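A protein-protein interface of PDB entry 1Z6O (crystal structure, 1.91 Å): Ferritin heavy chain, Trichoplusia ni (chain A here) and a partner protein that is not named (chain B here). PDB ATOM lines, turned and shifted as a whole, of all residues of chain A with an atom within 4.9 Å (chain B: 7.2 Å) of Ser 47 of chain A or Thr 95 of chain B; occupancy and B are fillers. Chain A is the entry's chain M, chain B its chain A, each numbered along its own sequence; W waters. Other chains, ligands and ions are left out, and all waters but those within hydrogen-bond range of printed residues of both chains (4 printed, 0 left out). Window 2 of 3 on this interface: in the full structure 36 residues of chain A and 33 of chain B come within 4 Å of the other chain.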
ATOM      1  N   GLY A  43      12.969   6.238  11.839  1.00  0.00           N
ATOM      2  CA  GLY A  43      12.088   6.484  10.702  1.00  0.00           C
ATOM      3  C   GLY A  43      12.471   7.790  10.011  1.00  0.00           C
ATOM      4  O   GLY A  43      12.520   7.876   8.779  1.00  0.00           O
ATOM      5  N   ALA A  44      12.746   8.818  10.808  1.00  0.00           N
ATOM      6  CA  ALA A  44      13.136  10.123  10.265  1.00  0.00           C
ATOM      7  C   ALA A  44      14.438  10.017   9.459  1.00  0.00           C
ATOM      8  O   ALA A  44      14.566  10.608   8.386  1.00  0.00           O
ATOM      9  CB  ALA A  44      13.323  11.131  11.414  1.00  0.00           C
ATOM     10  N   HIS A  45      15.409   9.276   9.982  1.00  0.00           N
ATOM     11  CA  HIS A  45      16.690   9.128   9.288  1.00  0.00           C
ATOM     12  C   HIS A  45      16.537   8.477   7.914  1.00  0.00           C
ATOM     13  O   HIS A  45      17.073   8.971   6.922  1.00  0.00           O
ATOM     14  CB  HIS A  45      17.664   8.286  10.131  1.00  0.00           C
ATOM     15  CG  HIS A  45      18.938   7.951   9.413  1.00  0.00           C
ATOM     16  ND1 HIS A  45      20.001   8.827   9.333  1.00  0.00           N
ATOM     17  CD2 HIS A  45      19.299   6.854   8.703  1.00  0.00           C
ATOM     18  CE1 HIS A  45      20.963   8.284   8.605  1.00  0.00           C
ATOM     19  NE2 HIS A  45      20.563   7.086   8.210  1.00  0.00           N
ATOM     20  N   PHE A  46      15.812   7.366   7.842  1.00  0.00           N
ATOM     21  CA  PHE A  46      15.667   6.696   6.556  1.00  0.00           C
ATOM     22  C   PHE A  46      14.732   7.399   5.585  1.00  0.00           C
ATOM     23  O   PHE A  46      14.671   7.036   4.410  1.00  0.00           O
ATOM     24  CB  PHE A  46      15.284   5.220   6.764  1.00  0.00           C
ATOM     25  CG  PHE A  46      16.408   4.408   7.369  1.00  0.00           C
ATOM     26  CD1 PHE A  46      16.433   4.136   8.733  1.00  0.00           C
ATOM     27  CD2 PHE A  46      17.498   4.020   6.581  1.00  0.00           C
ATOM     28  CE1 PHE A  46      17.537   3.491   9.318  1.00  0.00           C
ATOM     29  CE2 PHE A  46      18.611   3.374   7.149  1.00  0.00           C
ATOM     30  CZ  PHE A  46      18.630   3.110   8.519  1.00  0.00           C
ATOM     31  N   SER A  47      14.024   8.419   6.073  1.00  0.00           N
ATOM     32  CA  SER A  47      13.136   9.222   5.230  1.00  0.00           C
ATOM     33  C   SER A  47      13.916  10.335   4.511  1.00  0.00           C
ATOM     34  O   SER A  47      13.400  10.938   3.573  1.00  0.00           O
ATOM     35  CB  SER A  47      12.035   9.888   6.073  1.00  0.00           C
ATOM     36  OG  SER A  47      11.150   8.918   6.601  1.00  0.00           O
ATOM     37  N   LYS A  48      15.140  10.626   4.951  1.00  0.00           N
ATOM     38  CA  LYS A  48      15.926  11.698   4.316  1.00  0.00           C
ATOM     39  C   LYS A  48      16.177  11.444   2.834  1.00  0.00           C
ATOM     40  O   LYS A  48      16.402  10.303   2.422  1.00  0.00           O
ATOM     41  CB  LYS A  48      17.278  11.885   5.016  1.00  0.00           C
ATOM     42  CG  LYS A  48      17.165  12.327   6.471  1.00  0.00           C
ATOM     43  CD  LYS A  48      18.508  12.814   7.027  1.00  0.00           C
ATOM     44  CE  LYS A  48      19.594  11.774   6.901  1.00  0.00           C
ATOM     45  NZ  LYS A  48      20.874  12.241   7.519  1.00  0.00           N
ATOM     46  N   ASP A  49      16.161  12.512   2.038  1.00  0.00           N
ATOM     47  CA  ASP A  49      16.379  12.377   0.599  1.00  0.00           C
ATOM     48  C   ASP A  49      17.737  11.758   0.267  1.00  0.00           C
ATOM     49  O   ASP A  49      17.861  11.007  -0.709  1.00  0.00           O
ATOM     50  CB  ASP A  49      16.237  13.745  -0.101  1.00  0.00           C
ATOM     51  CG  ASP A  49      17.184  14.818   0.468  1.00  0.00           C
ATOM     52  OD1 ASP A  49      17.987  14.529   1.396  1.00  0.00           O
ATOM     53  OD2 ASP A  49      17.120  15.969  -0.018  1.00  0.00           O
ATOM     54  N   ALA A  57      12.217   3.180   6.514  1.00  0.00           N
ATOM     55  CA  ALA A  57      11.505   4.264   7.194  1.00  0.00           C
ATOM     56  C   ALA A  57      10.157   3.769   7.709  1.00  0.00           C
ATOM     57  O   ALA A  57       9.807   3.996   8.866  1.00  0.00           O
ATOM     58  CB  ALA A  57      11.294   5.457   6.244  1.00  0.00           C
ATOM     59  N   PHE A  61       8.807   3.540  11.555  1.00  0.00           N
ATOM     60  CA  PHE A  61       7.670   4.356  12.000  1.00  0.00           C
ATOM     61  C   PHE A  61       6.613   3.378  12.551  1.00  0.00           C
ATOM     62  O   PHE A  61       5.953   3.676  13.544  1.00  0.00           O
ATOM     63  CB  PHE A  61       7.068   5.172  10.844  1.00  0.00           C
ATOM     64  CG  PHE A  61       7.833   6.442  10.530  1.00  0.00           C
ATOM     65  CD1 PHE A  61       8.149   6.775   9.214  1.00  0.00           C
ATOM     66  CD2 PHE A  61       8.216   7.314  11.550  1.00  0.00           C
ATOM     67  CE1 PHE A  61       8.837   7.967   8.914  1.00  0.00           C
ATOM     68  CE2 PHE A  61       8.904   8.506  11.262  1.00  0.00           C
ATOM     69  CZ  PHE A  61       9.213   8.831   9.936  1.00  0.00           C
ATOM     70  N   ALA B  26      16.567  17.377  -2.326  1.00  0.00           N
ATOM     71  CA  ALA B  26      15.222  17.887  -2.570  1.00  0.00           C
ATOM     72  C   ALA B  26      15.018  19.342  -2.150  1.00  0.00           C
ATOM     73  O   ALA B  26      13.888  19.815  -2.088  1.00  0.00           O
ATOM     74  CB  ALA B  26      14.202  16.987  -1.856  1.00  0.00           C
ATOM     75  N   TYR B  31      14.893  26.524   0.784  1.00  0.00           N
ATOM     76  CA  TYR B  31      14.291  26.024   2.016  1.00  0.00           C
ATOM     77  C   TYR B  31      15.399  25.761   3.032  1.00  0.00           C
ATOM     78  O   TYR B  31      16.358  25.049   2.738  1.00  0.00           O
ATOM     79  CB  TYR B  31      13.557  24.709   1.739  1.00  0.00           C
ATOM     80  CG  TYR B  31      12.849  24.145   2.941  1.00  0.00           C
ATOM     81  CD1 TYR B  31      11.617  24.651   3.342  1.00  0.00           C
ATOM     82  CD2 TYR B  31      13.413  23.112   3.681  1.00  0.00           C
ATOM     83  CE1 TYR B  31      10.960  24.144   4.450  1.00  0.00           C
ATOM     84  CE2 TYR B  31      12.762  22.592   4.801  1.00  0.00           C
ATOM     85  CZ  TYR B  31      11.534  23.120   5.175  1.00  0.00           C
ATOM     86  OH  TYR B  31      10.889  22.633   6.282  1.00  0.00           O
ATOM     87  N   LEU B  41       9.365  24.254  11.663  1.00  0.00           N
ATOM     88  CA  LEU B  41       8.578  23.075  11.308  1.00  0.00           C
ATOM     89  C   LEU B  41       9.057  21.882  12.140  1.00  0.00           C
ATOM     90  O   LEU B  41       8.253  21.074  12.611  1.00  0.00           O
ATOM     91  CB  LEU B  41       8.703  22.778   9.813  1.00  0.00           C
ATOM     92  CG  LEU B  41       7.678  21.755   9.296  1.00  0.00           C
ATOM     93  CD1 LEU B  41       6.254  22.321   9.475  1.00  0.00           C
ATOM     94  CD2 LEU B  41       7.956  21.434   7.820  1.00  0.00           C
ATOM     95  N   ILE B  88       4.257  12.327  12.965  1.00  0.00           N
ATOM     96  CA  ILE B  88       4.882  11.566  11.891  1.00  0.00           C
ATOM     97  C   ILE B  88       4.729  12.280  10.548  1.00  0.00           C
ATOM     98  O   ILE B  88       5.664  12.320   9.744  1.00  0.00           O
ATOM     99  CB  ILE B  88       4.295  10.140  11.836  1.00  0.00           C
ATOM    100  CG1 ILE B  88       4.744   9.370  13.091  1.00  0.00           C
ATOM    101  CG2 ILE B  88       4.778   9.404  10.570  1.00  0.00           C
ATOM    102  CD1 ILE B  88       4.024   8.034  13.284  1.00  0.00           C
ATOM    103  N   ASP B  89       3.559  12.857  10.313  1.00  0.00           N
ATOM    104  CA  ASP B  89       3.322  13.581   9.069  1.00  0.00           C
ATOM    105  C   ASP B  89       4.281  14.774   8.922  1.00  0.00           C
ATOM    106  O   ASP B  89       4.815  15.017   7.838  1.00  0.00           O
ATOM    107  CB  ASP B  89       1.877  14.092   9.010  1.00  0.00           C
ATOM    108  CG  ASP B  89       1.516  14.635   7.628  1.00  0.00           C
ATOM    109  OD1 ASP B  89       1.372  15.866   7.467  1.00  0.00           O
ATOM    110  OD2 ASP B  89       1.398  13.819   6.691  1.00  0.00           O
ATOM    111  N   ILE B  90       4.500  15.522  10.000  1.00  0.00           N
ATOM    112  CA  ILE B  90       5.409  16.673   9.919  1.00  0.00           C
ATOM    113  C   ILE B  90       6.847  16.210   9.682  1.00  0.00           C
ATOM    114  O   ILE B  90       7.578  16.814   8.898  1.00  0.00           O
ATOM    115  CB  ILE B  90       5.343  17.529  11.204  1.00  0.00           C
ATOM    116  CG1 ILE B  90       3.950  18.163  11.325  1.00  0.00           C
ATOM    117  CG2 ILE B  90       6.415  18.650  11.159  1.00  0.00           C
ATOM    118  CD1 ILE B  90       3.633  18.670  12.753  1.00  0.00           C
ATOM    119  N   ILE B  91       7.258  15.143  10.362  1.00  0.00           N
ATOM    120  CA  ILE B  91       8.606  14.609  10.162  1.00  0.00           C
ATOM    121  C   ILE B  91       8.780  14.244   8.686  1.00  0.00           C
ATOM    122  O   ILE B  91       9.815  14.527   8.082  1.00  0.00           O
ATOM    123  CB  ILE B  91       8.848  13.351  11.042  1.00  0.00           C
ATOM    124  CG1 ILE B  91       8.990  13.771  12.513  1.00  0.00           C
ATOM    125  CG2 ILE B  91      10.109  12.593  10.560  1.00  0.00           C
ATOM    126  CD1 ILE B  91       8.954  12.584  13.497  1.00  0.00           C
ATOM    127  N   LYS B  92       7.769  13.613   8.101  1.00  0.00           N
ATOM    128  CA  LYS B  92       7.848  13.249   6.690  1.00  0.00           C
ATOM    129  C   LYS B  92       7.885  14.490   5.797  1.00  0.00           C
ATOM    130  O   LYS B  92       8.552  14.485   4.761  1.00  0.00           O
ATOM    131  CB  LYS B  92       6.671  12.352   6.288  1.00  0.00           C
ATOM    132  CG  LYS B  92       6.775  10.928   6.884  1.00  0.00           C
ATOM    133  CD  LYS B  92       5.553  10.091   6.527  1.00  0.00           C
ATOM    134  CE  LYS B  92       5.732   8.644   7.005  1.00  0.00           C
ATOM    135  NZ  LYS B  92       4.495   7.828   6.760  1.00  0.00           N
ATOM    136  N   HIS B  93       7.188  15.557   6.186  1.00  0.00           N
ATOM    137  CA  HIS B  93       7.211  16.768   5.364  1.00  0.00           C
ATOM    138  C   HIS B  93       8.589  17.439   5.418  1.00  0.00           C
ATOM    139  O   HIS B  93       9.094  17.940   4.409  1.00  0.00           O
ATOM    140  CB  HIS B  93       6.147  17.776   5.821  1.00  0.00           C
ATOM    141  CG  HIS B  93       5.782  18.758   4.753  1.00  0.00           C
ATOM    142  ND1 HIS B  93       4.806  18.501   3.815  1.00  0.00           N
ATOM    143  CD2 HIS B  93       6.327  19.951   4.412  1.00  0.00           C
ATOM    144  CE1 HIS B  93       4.766  19.492   2.939  1.00  0.00           C
ATOM    145  NE2 HIS B  93       5.680  20.385   3.278  1.00  0.00           N
ATOM    146  N   VAL B  94       9.182  17.462   6.606  1.00  0.00           N
ATOM    147  CA  VAL B  94      10.520  18.026   6.807  1.00  0.00           C
ATOM    148  C   VAL B  94      11.510  17.319   5.859  1.00  0.00           C
ATOM    149  O   VAL B  94      12.321  17.969   5.178  1.00  0.00           O
ATOM    150  CB  VAL B  94      10.974  17.823   8.294  1.00  0.00           C
ATOM    151  CG1 VAL B  94      12.494  18.001   8.437  1.00  0.00           C
ATOM    152  CG2 VAL B  94      10.230  18.821   9.202  1.00  0.00           C
ATOM    153  N   THR B  95      11.443  15.991   5.799  1.00  0.00           N
ATOM    154  CA  THR B  95      12.360  15.257   4.923  1.00  0.00           C
ATOM    155  C   THR B  95      11.966  15.365   3.455  1.00  0.00           C
ATOM    156  O   THR B  95      12.828  15.321   2.576  1.00  0.00           O
ATOM    157  CB  THR B  95      12.474  13.770   5.318  1.00  0.00           C
ATOM    158  OG1 THR B  95      11.184  13.152   5.272  1.00  0.00           O
ATOM    159  CG2 THR B  95      13.053  13.648   6.728  1.00  0.00           C
ATOM    160  N   LYS B  96      10.673  15.505   3.182  1.00  0.00           N
ATOM    161  CA  LYS B  96      10.235  15.665   1.794  1.00  0.00           C
ATOM    162  C   LYS B  96      10.872  16.931   1.200  1.00  0.00           C
ATOM    163  O   LYS B  96      11.247  16.958   0.025  1.00  0.00           O
ATOM    164  CB  LYS B  96       8.704  15.796   1.718  1.00  0.00           C
ATOM    165  CG  LYS B  96       8.210  16.107   0.299  1.00  0.00           C
ATOM    166  CD  LYS B  96       6.708  15.856   0.116  1.00  0.00           C
ATOM    167  CE  LYS B  96       5.872  16.815   0.926  1.00  0.00           C
ATOM    168  NZ  LYS B  96       4.413  16.550   0.718  1.00  0.00           N
ATOM    169  N   ARG B  97      10.993  17.978   2.019  1.00  0.00           N
ATOM    170  CA  ARG B  97      11.575  19.241   1.566  1.00  0.00           C
ATOM    171  C   ARG B  97      13.108  19.274   1.635  1.00  0.00           C
ATOM    172  O   ARG B  97      13.720  20.335   1.507  1.00  0.00           O
ATOM    173  CB  ARG B  97      10.966  20.425   2.347  1.00  0.00           C
ATOM    174  CG  ARG B  97       9.453  20.645   2.076  1.00  0.00           C
ATOM    175  CD  ARG B  97       9.167  20.928   0.582  1.00  0.00           C
ATOM    176  NE  ARG B  97       9.966  22.043   0.071  1.00  0.00           N
ATOM    177  CZ  ARG B  97       9.675  23.331   0.241  1.00  0.00           C
ATOM    178  NH1 ARG B  97       8.583  23.701   0.906  1.00  0.00           N
ATOM    179  NH2 ARG B  97      10.497  24.258  -0.236  1.00  0.00           N
ATOM    180  N   GLY B  98      13.726  18.114   1.855  1.00  0.00           N
ATOM    181  CA  GLY B  98      15.182  18.042   1.843  1.00  0.00           C
ATOM    182  C   GLY B  98      15.929  18.371   3.114  1.00  0.00           C
ATOM    183  O   GLY B  98      17.141  18.533   3.098  1.00  0.00           O
ATOM    184  N   ASP B  99      15.218  18.446   4.226  1.00  0.00           N
ATOM    185  CA  ASP B  99      15.844  18.780   5.500  1.00  0.00           C
ATOM    186  C   ASP B  99      15.918  17.492   6.323  1.00  0.00           C
ATOM    187  O   ASP B  99      15.604  16.403   5.830  1.00  0.00           O
ATOM    188  CB  ASP B  99      14.969  19.841   6.185  1.00  0.00           C
ATOM    189  CG  ASP B  99      15.665  20.564   7.331  1.00  0.00           C
ATOM    190  OD1 ASP B  99      16.871  20.346   7.570  1.00  0.00           O
ATOM    191  OD2 ASP B  99      14.974  21.370   7.996  1.00  0.00           O
ATOM    192  N   LYS B 100      16.376  17.595   7.559  1.00  0.00           N
ATOM    193  CA  LYS B 100      16.420  16.423   8.414  1.00  0.00           C
ATOM    194  C   LYS B 100      15.850  16.822   9.756  1.00  0.00           C
ATOM    195  O   LYS B 100      16.036  17.948  10.217  1.00  0.00           O
ATOM    196  CB  LYS B 100      17.839  15.881   8.560  1.00  0.00           C
ATOM    197  CG  LYS B 100      18.789  16.710   9.356  1.00  0.00           C
ATOM    198  CD  LYS B 100      20.101  15.945   9.484  1.00  0.00           C
ATOM    199  CE  LYS B 100      21.189  16.788  10.121  1.00  0.00           C
ATOM    200  NZ  LYS B 100      22.509  16.097  10.067  1.00  0.00           N
ATOM    201  N   MET B 101      15.138  15.897  10.371  1.00  0.00           N
ATOM    202  CA  MET B 101      14.497  16.154  11.643  1.00  0.00           C
ATOM    203  C   MET B 101      15.499  16.177  12.791  1.00  0.00           C
ATOM    204  O   MET B 101      16.372  15.329  12.875  1.00  0.00           O
ATOM    205  CB  MET B 101      13.433  15.080  11.889  1.00  0.00           C
ATOM    206  CG  MET B 101      12.682  15.223  13.194  1.00  0.00           C
ATOM    207  SD  MET B 101      11.770  16.794  13.280  1.00  0.00           S
ATOM    208  CE  MET B 101      11.404  16.827  15.009  1.00  0.00           C
HETATM  209  O   HOH W   1      15.365  13.281   9.298  1.00  0.00           O
HETATM  210  O   HOH W   2      18.867  16.999   1.995  1.00  0.00           O
HETATM  211  O   HOH W   3      10.935  12.042   2.560  1.00  0.00           O
HETATM  212  O   HOH W   4      15.438  15.019   3.306  1.00  0.00           O
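The backbone NH (N) of Ala 26 of chain B is in hydrogen-bond range of the side-chain carboxylate (OD2) of Asp 49 of chain A (2.8 Å).
The side-chain hydroxyl (OG1) of Thr 95 of chain B sits at hydrogen-bond distance from the backbone carbonyl oxygen (O) of Ile 91 of chain B, 3.4 Å away.
O of Lys 92 of chain B sits at hydrogen-bond distance from OG1 of Thr 95 of chain B, 3.0 Å away.
O of Gly 43 of chain A lies within hydrogen-bond range of OG of Ser 47 of chain A (2.8 Å).
CB of Ala 44 of chain A touches CG2 of Ile 91 of chain B (3.6 Å).
O of Ala 44 of chain A touches CG2 of Thr 95 of chain B, 3.8 Å away.
Ala 44 of chain A touches Met 101 of chain B.
Ser 47 of chain A touches Thr 95 of chain B (O to CB, 3.5 Å).
Lys 48 of chain A touches Lys 100 of chain B.
Asp 49 of chain A touches Gly 98 of chain B (OD2 to CA, 3.4 Å).
CZ of Phe 61 of chain A touches CG2 of Ile 91 of chain B (3.9 Å).
Phe 61 of chain A touches Lys 92 of chain B.
Ser 47 of chain A touches just one residue of chain B: Thr 95.
Printed residues of chain B within 4 Å of Lys 48 of chain A: Lys 100.
Of the printed residues of chain B, Asp 49 of chain A touches Ala 26 and Gly 98.
Printed residues of chain A within 4 Å of Ile 91 of chain B: Ala 44 (3.6 Å) and Phe 61 (3.9 Å).
Of the printed residues of chain A, Lys 92 of chain B touches Phe 61 (3.7 Å).
Thr 95 of chain B touches just these residues of chain A: Ala 44 (3.8 Å) and Ser 47 (3.5 Å).
Of the printed residues of chain A, Lys 100 of chain B touches Lys 48.
Hydrophobic or aromatic side chains of chain A within 4 Å of the printed part of chain B: Ala 44 and Phe 61.
Of the 17 printed residues of chain B, 7 touch a printed residue of chain A.
Hydrophobic or aromatic side chains of chain B within 4 Å of the printed part of chain A: Ala 26, Ile 91 and Met 101.
Among the printed residues, 9 pairs touch across the chains.
Among the printed residues, no Asp or Glu carboxylate lies within 4 Å of a Lys or Arg side-chain nitrogen of the other chain.
Water W2 bridges O of Gly 98 of chain B (2.6 Å) and OD1 of Asp 49 of chain A (2.7 Å).
Water W4 lies within hydrogen-bond range of O of Thr 95 of chain B, O of Asp 99 of chain B and N of Asp 49 of chain A.
Water W1 bridges the backbone NH (N) of Met 101 of chain B (2.8 Å) and the backbone carbonyl oxygen (O) of Ala 44 of chain A (2.9 Å).
Water W3 lies within hydrogen-bond range of O of Ser 47 of chain A (2.9 Å) and OG1 of Thr 95 of chain B (2.9 Å).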
